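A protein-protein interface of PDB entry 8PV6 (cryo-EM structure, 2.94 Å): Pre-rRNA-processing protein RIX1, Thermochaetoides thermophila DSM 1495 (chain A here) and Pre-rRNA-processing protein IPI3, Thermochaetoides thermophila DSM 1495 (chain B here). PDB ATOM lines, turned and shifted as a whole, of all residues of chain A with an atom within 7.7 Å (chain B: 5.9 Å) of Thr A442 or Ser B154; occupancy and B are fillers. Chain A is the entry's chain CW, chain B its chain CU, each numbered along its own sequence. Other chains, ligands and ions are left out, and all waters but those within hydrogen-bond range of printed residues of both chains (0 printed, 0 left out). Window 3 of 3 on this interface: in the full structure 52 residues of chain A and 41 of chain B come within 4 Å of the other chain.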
ATOM      1  N   ILE A 401       2.462  19.762  11.184  1.00  0.00           N
ATOM      2  CA  ILE A 401       1.584  20.937  11.243  1.00  0.00           C
ATOM      3  C   ILE A 401       2.303  22.245  10.921  1.00  0.00           C
ATOM      4  O   ILE A 401       1.715  23.078  10.215  1.00  0.00           O
ATOM      5  CB  ILE A 401       0.835  20.966  12.583  1.00  0.00           C
ATOM      6  CG1 ILE A 401       0.009  19.693  12.755  1.00  0.00           C
ATOM      7  CG2 ILE A 401      -0.077  22.166  12.680  1.00  0.00           C
ATOM      8  CD1 ILE A 401      -0.795  19.649  14.038  1.00  0.00           C
ATOM      9  N   PRO A 402       3.537  22.518  11.395  1.00  0.00           N
ATOM     10  CA  PRO A 402       4.219  23.744  10.932  1.00  0.00           C
ATOM     11  C   PRO A 402       4.448  23.813   9.431  1.00  0.00           C
ATOM     12  O   PRO A 402       4.465  24.914   8.870  1.00  0.00           O
ATOM     13  CB  PRO A 402       5.549  23.709  11.693  1.00  0.00           C
ATOM     14  CG  PRO A 402       5.234  23.013  12.928  1.00  0.00           C
ATOM     15  CD  PRO A 402       4.279  21.933  12.534  1.00  0.00           C
ATOM     16  N   ALA A 404       2.358  22.690   7.215  1.00  0.00           N
ATOM     17  CA  ALA A 404       1.088  22.449   6.531  1.00  0.00           C
ATOM     18  C   ALA A 404       0.685  23.607   5.628  1.00  0.00           C
ATOM     19  O   ALA A 404       0.120  23.388   4.552  1.00  0.00           O
ATOM     20  CB  ALA A 404      -0.013  22.171   7.554  1.00  0.00           C
ATOM     21  N   THR A 405       0.954  24.845   6.053  1.00  0.00           N
ATOM     22  CA  THR A 405       0.530  26.008   5.276  1.00  0.00           C
ATOM     23  C   THR A 405       1.259  26.084   3.938  1.00  0.00           C
ATOM     24  O   THR A 405       0.661  26.444   2.916  1.00  0.00           O
ATOM     25  CB  THR A 405       0.755  27.287   6.082  1.00  0.00           C
ATOM     26  OG1 THR A 405       0.207  27.124   7.396  1.00  0.00           O
ATOM     27  CG2 THR A 405       0.076  28.471   5.409  1.00  0.00           C
ATOM     28  N   LEU A 436      -5.696  17.938   5.133  1.00  0.00           N
ATOM     29  CA  LEU A 436      -6.933  18.307   5.805  1.00  0.00           C
ATOM     30  C   LEU A 436      -7.229  17.410   6.996  1.00  0.00           C
ATOM     31  O   LEU A 436      -7.793  17.891   7.984  1.00  0.00           O
ATOM     32  CB  LEU A 436      -8.095  18.286   4.813  1.00  0.00           C
ATOM     33  CG  LEU A 436      -8.091  19.388   3.750  1.00  0.00           C
ATOM     34  CD1 LEU A 436      -9.367  19.346   2.932  1.00  0.00           C
ATOM     35  CD2 LEU A 436      -7.895  20.755   4.375  1.00  0.00           C
ATOM     36  N   LEU A 438      -4.789  16.322   8.797  1.00  0.00           N
ATOM     37  CA  LEU A 438      -3.804  16.741   9.785  1.00  0.00           C
ATOM     38  C   LEU A 438      -4.200  18.046  10.464  1.00  0.00           C
ATOM     39  O   LEU A 438      -4.459  18.067  11.671  1.00  0.00           O
ATOM     40  CB  LEU A 438      -2.432  16.887   9.132  1.00  0.00           C
ATOM     41  CG  LEU A 438      -1.321  17.171  10.133  1.00  0.00           C
ATOM     42  CD1 LEU A 438      -1.226  16.001  11.082  1.00  0.00           C
ATOM     43  CD2 LEU A 438       0.000  17.404   9.423  1.00  0.00           C
ATOM     44  N   ALA A 439      -4.255  19.136   9.702  1.00  0.00           N
ATOM     45  CA  ALA A 439      -4.666  20.447  10.206  1.00  0.00           C
ATOM     46  C   ALA A 439      -5.613  21.074   9.189  1.00  0.00           C
ATOM     47  O   ALA A 439      -5.194  21.835   8.316  1.00  0.00           O
ATOM     48  CB  ALA A 439      -3.453  21.330  10.465  1.00  0.00           C
ATOM     49  N   GLY A 440      -6.899  20.760   9.315  1.00  0.00           N
ATOM     50  CA  GLY A 440      -7.890  21.268   8.387  1.00  0.00           C
ATOM     51  C   GLY A 440      -9.049  21.982   9.049  1.00  0.00           C
ATOM     52  O   GLY A 440      -9.714  22.811   8.423  1.00  0.00           O
ATOM     53  N   SER A 441      -9.299  21.673  10.322  1.00  0.00           N
ATOM     54  CA  SER A 441     -10.462  22.211  11.015  1.00  0.00           C
ATOM     55  C   SER A 441     -10.266  23.643  11.492  1.00  0.00           C
ATOM     56  O   SER A 441     -11.217  24.238  12.008  1.00  0.00           O
ATOM     57  CB  SER A 441     -10.820  21.319  12.202  1.00  0.00           C
ATOM     58  OG  SER A 441      -9.689  21.085  13.022  1.00  0.00           O
ATOM     59  N   THR A 442      -9.066  24.207  11.342  1.00  0.00           N
ATOM     60  CA  THR A 442      -8.805  25.585  11.740  1.00  0.00           C
ATOM     61  C   THR A 442      -8.206  26.400  10.600  1.00  0.00           C
ATOM     62  O   THR A 442      -7.418  27.316  10.850  1.00  0.00           O
ATOM     63  CB  THR A 442      -7.880  25.636  12.956  1.00  0.00           C
ATOM     64  OG1 THR A 442      -6.797  24.716  12.772  1.00  0.00           O
ATOM     65  CG2 THR A 442      -8.640  25.271  14.215  1.00  0.00           C
ATOM     66  N   LEU A 443      -8.555  26.082   9.359  1.00  0.00           N
ATOM     67  CA  LEU A 443      -8.031  26.833   8.231  1.00  0.00           C
ATOM     68  C   LEU A 443      -8.697  28.205   8.162  1.00  0.00           C
ATOM     69  O   LEU A 443      -9.883  28.338   8.488  1.00  0.00           O
ATOM     70  CB  LEU A 443      -8.261  26.074   6.926  1.00  0.00           C
ATOM     71  CG  LEU A 443      -7.258  24.968   6.609  1.00  0.00           C
ATOM     72  CD1 LEU A 443      -7.569  24.365   5.260  1.00  0.00           C
ATOM     73  CD2 LEU A 443      -5.836  25.506   6.641  1.00  0.00           C
ATOM     74  N   PRO A 444      -7.974  29.240   7.750  1.00  0.00           N
ATOM     75  CA  PRO A 444      -8.595  30.555   7.589  1.00  0.00           C
ATOM     76  C   PRO A 444      -9.441  30.638   6.329  1.00  0.00           C
ATOM     77  O   PRO A 444      -9.399  29.764   5.455  1.00  0.00           O
ATOM     78  CB  PRO A 444      -7.394  31.505   7.517  1.00  0.00           C
ATOM     79  CG  PRO A 444      -6.296  30.670   6.981  1.00  0.00           C
ATOM     80  CD  PRO A 444      -6.523  29.278   7.498  1.00  0.00           C
ATOM     81  N   LYS A 445     -10.210  31.725   6.252  1.00  0.00           N
ATOM     82  CA  LYS A 445     -11.171  31.966   5.182  1.00  0.00           C
ATOM     83  C   LYS A 445     -10.494  32.017   3.818  1.00  0.00           C
ATOM     84  O   LYS A 445     -11.025  31.484   2.839  1.00  0.00           O
ATOM     85  CB  LYS A 445     -11.932  33.267   5.448  1.00  0.00           C
ATOM     86  CG  LYS A 445     -12.842  33.715   4.317  1.00  0.00           C
ATOM     87  CD  LYS A 445     -14.169  32.979   4.350  1.00  0.00           C
ATOM     88  CE  LYS A 445     -15.100  33.477   3.258  1.00  0.00           C
ATOM     89  NZ  LYS A 445     -16.435  32.822   3.327  1.00  0.00           N
ATOM     90  N   THR A 447      -7.710  30.486   2.934  1.00  0.00           N
ATOM     91  CA  THR A 447      -7.289  29.144   2.540  1.00  0.00           C
ATOM     92  C   THR A 447      -8.480  28.295   2.107  1.00  0.00           C
ATOM     93  O   THR A 447      -8.390  27.542   1.126  1.00  0.00           O
ATOM     94  CB  THR A 447      -6.524  28.478   3.683  1.00  0.00           C
ATOM     95  OG1 THR A 447      -5.456  29.337   4.100  1.00  0.00           O
ATOM     96  CG2 THR A 447      -5.936  27.150   3.237  1.00  0.00           C
ATOM     97  N   VAL A 448      -9.612  28.419   2.808  1.00  0.00           N
ATOM     98  CA  VAL A 448     -10.824  27.734   2.367  1.00  0.00           C
ATOM     99  C   VAL A 448     -11.272  28.229   0.995  1.00  0.00           C
ATOM    100  O   VAL A 448     -11.709  27.426   0.162  1.00  0.00           O
ATOM    101  CB  VAL A 448     -11.948  27.890   3.411  1.00  0.00           C
ATOM    102  CG1 VAL A 448     -13.191  27.129   2.986  1.00  0.00           C
ATOM    103  CG2 VAL A 448     -11.486  27.382   4.760  1.00  0.00           C
ATOM    104  N   HIS A 531     -13.465  17.794   8.048  1.00  0.00           N
ATOM    105  CA  HIS A 531     -12.288  18.561   8.428  1.00  0.00           C
ATOM    106  C   HIS A 531     -12.145  19.861   7.651  1.00  0.00           C
ATOM    107  O   HIS A 531     -11.037  20.196   7.220  1.00  0.00           O
ATOM    108  CB  HIS A 531     -11.034  17.709   8.253  1.00  0.00           C
ATOM    109  CG  HIS A 531     -10.883  16.639   9.287  1.00  0.00           C
ATOM    110  ND1 HIS A 531     -11.397  15.371   9.124  1.00  0.00           N
ATOM    111  CD2 HIS A 531     -10.284  16.649  10.499  1.00  0.00           C
ATOM    112  CE1 HIS A 531     -11.117  14.645  10.190  1.00  0.00           C
ATOM    113  NE2 HIS A 531     -10.442  15.397  11.041  1.00  0.00           N
ATOM    114  N   LEU A 532     -13.232  20.597   7.456  1.00  0.00           N
ATOM    115  CA  LEU A 532     -13.179  21.911   6.850  1.00  0.00           C
ATOM    116  C   LEU A 532     -14.143  22.830   7.584  1.00  0.00           C
ATOM    117  O   LEU A 532     -15.198  22.369   8.042  1.00  0.00           O
ATOM    118  CB  LEU A 532     -13.542  21.839   5.358  1.00  0.00           C
ATOM    119  CG  LEU A 532     -12.816  22.781   4.398  1.00  0.00           C
ATOM    120  CD1 LEU A 532     -11.316  22.662   4.574  1.00  0.00           C
ATOM    121  CD2 LEU A 532     -13.206  22.480   2.966  1.00  0.00           C
ATOM    122  N   PRO A 533     -13.823  24.114   7.739  1.00  0.00           N
ATOM    123  CA  PRO A 533     -14.776  25.035   8.372  1.00  0.00           C
ATOM    124  C   PRO A 533     -15.980  25.274   7.473  1.00  0.00           C
ATOM    125  O   PRO A 533     -15.858  25.812   6.371  1.00  0.00           O
ATOM    126  CB  PRO A 533     -13.956  26.314   8.575  1.00  0.00           C
ATOM    127  CG  PRO A 533     -12.534  25.878   8.504  1.00  0.00           C
ATOM    128  CD  PRO A 533     -12.506  24.737   7.543  1.00  0.00           C
ATOM    129  N   HIS A 536     -16.901  28.941   6.458  1.00  0.00           N
ATOM    130  CA  HIS A 536     -16.137  29.618   5.417  1.00  0.00           C
ATOM    131  C   HIS A 536     -16.557  29.176   4.022  1.00  0.00           C
ATOM    132  O   HIS A 536     -16.195  29.825   3.035  1.00  0.00           O
ATOM    133  CB  HIS A 536     -14.644  29.374   5.626  1.00  0.00           C
ATOM    134  CG  HIS A 536     -14.120  29.918   6.917  1.00  0.00           C
ATOM    135  ND1 HIS A 536     -14.798  30.862   7.656  1.00  0.00           N
ATOM    136  CD2 HIS A 536     -12.982  29.653   7.600  1.00  0.00           C
ATOM    137  CE1 HIS A 536     -14.103  31.155   8.739  1.00  0.00           C
ATOM    138  NE2 HIS A 536     -12.995  30.434   8.730  1.00  0.00           N
ATOM    139  N   SER B 137      -6.340  20.174  17.399  1.00  0.00           N
ATOM    140  CA  SER B 137      -6.515  21.418  16.661  1.00  0.00           C
ATOM    141  C   SER B 137      -6.703  22.648  17.537  1.00  0.00           C
ATOM    142  O   SER B 137      -6.761  23.753  16.988  1.00  0.00           O
ATOM    143  CB  SER B 137      -7.708  21.307  15.706  1.00  0.00           C
ATOM    144  OG  SER B 137      -8.873  20.894  16.398  1.00  0.00           O
ATOM    145  N   HIS B 138      -6.800  22.524  18.862  1.00  0.00           N
ATOM    146  CA  HIS B 138      -7.088  23.671  19.712  1.00  0.00           C
ATOM    147  C   HIS B 138      -6.341  23.582  21.036  1.00  0.00           C
ATOM    148  O   HIS B 138      -6.027  22.499  21.532  1.00  0.00           O
ATOM    149  CB  HIS B 138      -8.589  23.803  19.992  1.00  0.00           C
ATOM    150  CG  HIS B 138      -9.380  24.293  18.822  1.00  0.00           C
ATOM    151  ND1 HIS B 138      -9.906  23.447  17.872  1.00  0.00           N
ATOM    152  CD2 HIS B 138      -9.731  25.544  18.446  1.00  0.00           C
ATOM    153  CE1 HIS B 138     -10.551  24.155  16.963  1.00  0.00           C
ATOM    154  NE2 HIS B 138     -10.460  25.431  17.288  1.00  0.00           N
ATOM    155  N   SER B 152      -5.673  28.375  18.113  1.00  0.00           N
ATOM    156  CA  SER B 152      -5.536  27.398  17.042  1.00  0.00           C
ATOM    157  C   SER B 152      -4.115  26.849  17.047  1.00  0.00           C
ATOM    158  O   SER B 152      -3.150  27.620  17.011  1.00  0.00           O
ATOM    159  CB  SER B 152      -5.865  28.022  15.689  1.00  0.00           C
ATOM    160  OG  SER B 152      -5.428  27.189  14.631  1.00  0.00           O
ATOM    161  N   LEU B 153      -3.993  25.521  17.091  1.00  0.00           N
ATOM    162  CA  LEU B 153      -2.677  24.890  17.144  1.00  0.00           C
ATOM    163  C   LEU B 153      -1.893  25.127  15.859  1.00  0.00           C
ATOM    164  O   LEU B 153      -0.686  25.399  15.899  1.00  0.00           O
ATOM    165  CB  LEU B 153      -2.829  23.394  17.406  1.00  0.00           C
ATOM    166  CG  LEU B 153      -1.575  22.679  17.902  1.00  0.00           C
ATOM    167  CD1 LEU B 153      -1.104  23.327  19.183  1.00  0.00           C
ATOM    168  CD2 LEU B 153      -1.843  21.201  18.111  1.00  0.00           C
ATOM    169  N   SER B 154      -2.565  25.030  14.709  1.00  0.00           N
ATOM    170  CA  SER B 154      -1.899  25.268  13.433  1.00  0.00           C
ATOM    171  C   SER B 154      -1.476  26.722  13.280  1.00  0.00           C
ATOM    172  O   SER B 154      -0.424  27.000  12.696  1.00  0.00           O
ATOM    173  CB  SER B 154      -2.812  24.856  12.281  1.00  0.00           C
ATOM    174  OG  SER B 154      -3.995  25.635  12.264  1.00  0.00           O
ATOM    175  N   GLN B 155      -2.277  27.656  13.791  1.00  0.00           N
ATOM    176  CA  GLN B 155      -1.912  29.064  13.766  1.00  0.00           C
ATOM    177  C   GLN B 155      -0.761  29.370  14.713  1.00  0.00           C
ATOM    178  O   GLN B 155       0.069  30.232  14.406  1.00  0.00           O
ATOM    179  CB  GLN B 155      -3.141  29.922  14.103  1.00  0.00           C
ATOM    180  CG  GLN B 155      -2.985  31.435  13.932  1.00  0.00           C
ATOM    181  CD  GLN B 155      -2.400  32.127  15.149  1.00  0.00           C
ATOM    182  OE1 GLN B 155      -2.580  31.676  16.279  1.00  0.00           O
ATOM    183  NE2 GLN B 155      -1.696  33.230  14.922  1.00  0.00           N
ATOM    184  N   LEU B 156      -0.696  28.687  15.858  1.00  0.00           N
ATOM    185  CA  LEU B 156       0.432  28.873  16.765  1.00  0.00           C
ATOM    186  C   LEU B 156       1.715  28.293  16.182  1.00  0.00           C
ATOM    187  O   LEU B 156       2.794  28.873  16.342  1.00  0.00           O
ATOM    188  CB  LEU B 156       0.129  28.241  18.123  1.00  0.00           C
ATOM    189  CG  LEU B 156      -0.892  28.963  19.001  1.00  0.00           C
ATOM    190  CD1 LEU B 156      -1.090  28.227  20.311  1.00  0.00           C
ATOM    191  CD2 LEU B 156      -0.456  30.387  19.255  1.00  0.00           C
ATOM    192  N   LEU B 157       1.619  27.153  15.503  1.00  0.00           N
ATOM    193  CA  LEU B 157       2.781  26.469  14.947  1.00  0.00           C
ATOM    194  C   LEU B 157       2.887  26.773  13.459  1.00  0.00           C
ATOM    195  O   LEU B 157       2.391  26.003  12.629  1.00  0.00           O
ATOM    196  CB  LEU B 157       2.690  24.960  15.169  1.00  0.00           C
ATOM    197  CG  LEU B 157       3.256  24.369  16.461  1.00  0.00           C
ATOM    198  CD1 LEU B 157       2.384  24.716  17.643  1.00  0.00           C
ATOM    199  CD2 LEU B 157       3.396  22.864  16.326  1.00  0.00           C
ATOM    200  N   GLU B 158       3.530  27.888  13.124  1.00  0.00           N
ATOM    201  CA  GLU B 158       3.854  28.210  11.744  1.00  0.00           C
ATOM    202  C   GLU B 158       5.332  28.539  11.646  1.00  0.00           C
ATOM    203  O   GLU B 158       5.896  29.166  12.547  1.00  0.00           O
ATOM    204  CB  GLU B 158       3.042  29.396  11.207  1.00  0.00           C
ATOM    205  CG  GLU B 158       1.569  29.388  11.544  1.00  0.00           C
ATOM    206  CD  GLU B 158       0.885  30.675  11.129  1.00  0.00           C
ATOM    207  OE1 GLU B 158       1.487  31.436  10.342  1.00  0.00           O
ATOM    208  OE2 GLU B 158      -0.251  30.926  11.580  1.00  0.00           O
ATOM    209  N   LEU B 168      -8.677  32.756  19.168  1.00  0.00           N
ATOM    210  CA  LEU B 168      -9.862  32.821  18.318  1.00  0.00           C
ATOM    211  C   LEU B 168     -11.062  33.377  19.072  1.00  0.00           C
ATOM    212  O   LEU B 168     -11.807  34.209  18.541  1.00  0.00           O
ATOM    213  CB  LEU B 168     -10.179  31.434  17.763  1.00  0.00           C
ATOM    214  CG  LEU B 168      -9.108  30.801  16.879  1.00  0.00           C
ATOM    215  CD1 LEU B 168      -9.501  29.387  16.498  1.00  0.00           C
ATOM    216  CD2 LEU B 168      -8.876  31.648  15.640  1.00  0.00           C
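Of the 19 printed residues of chain A, 4 touch a printed residue of chain B.
Hydrophobic or aromatic side chains of chain A within 4 Å of the printed part of chain B: Ile A401 and Pro A402.
Hydrophobic or aromatic side chains of chain B within 4 Å of the printed part of chain A: His B138 and Leu B157.
Among the printed residues, no Asp or Glu carboxylate lies within 4 Å of a Lys or Arg side-chain nitrogen of the other chain.
Of the printed residues of chain B, Ile A401 touches Ser B154 (3.7 Å) and Leu B157 (3.9 Å).
Printed residues of chain B within 4 Å of Pro A402: Leu B157.
Of chain B, only Ser B137 (3.7 Å), His B138 (3.5 Å), Ser B152 (3.4 Å) and Ser B154 (3.0 Å) come within 4 Å of Thr A442.
Pro A444 touches none of the printed residues of chain B.
Printed residues of chain A within 4 Å of Leu B157: Ile A401 (3.9 Å) and Pro A402 (3.4 Å).
The nearest printed residue of chain A that does not touch Ser B154 is Ala A439 (4.02 Å).
Among the printed residues, pairs that only touch across the chains: Pro A402 with Leu B157, Thr A442 with His B138, Ile A401 with Ser B154, Thr A442 with Ser B137 and Ile A401 with Leu B157.
OG of Ser A441 sits close to OG of Ser B137, at 3.5 Å.
The side-chain hydroxyl of Ser B152 lies close to the side-chain hydroxyl of Thr A442 (3.4 Å).
OG1 of Thr A442 sits at hydrogen-bond distance from OG of Ser B154, at 3.0 Å.
ND1 of His B138 lies within hydrogen-bond range of OG of Ser B137, at 3.1 Å.
The backbone carbonyl oxygen (O) of Ser B137 is in hydrogen-bond range of the backbone NH (N) of Leu B153 (3.3 Å).
The side-chain hydroxyl (OG) of Ser B152 lies within hydrogen-bond range of the side-chain hydroxyl (OG) of Ser B154 (3.2 Å).
The side-chain hydroxyl (OG) of Ser B152 is in hydrogen-bond range of the backbone NH (N) of Gln B155, 3.3 Å away.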
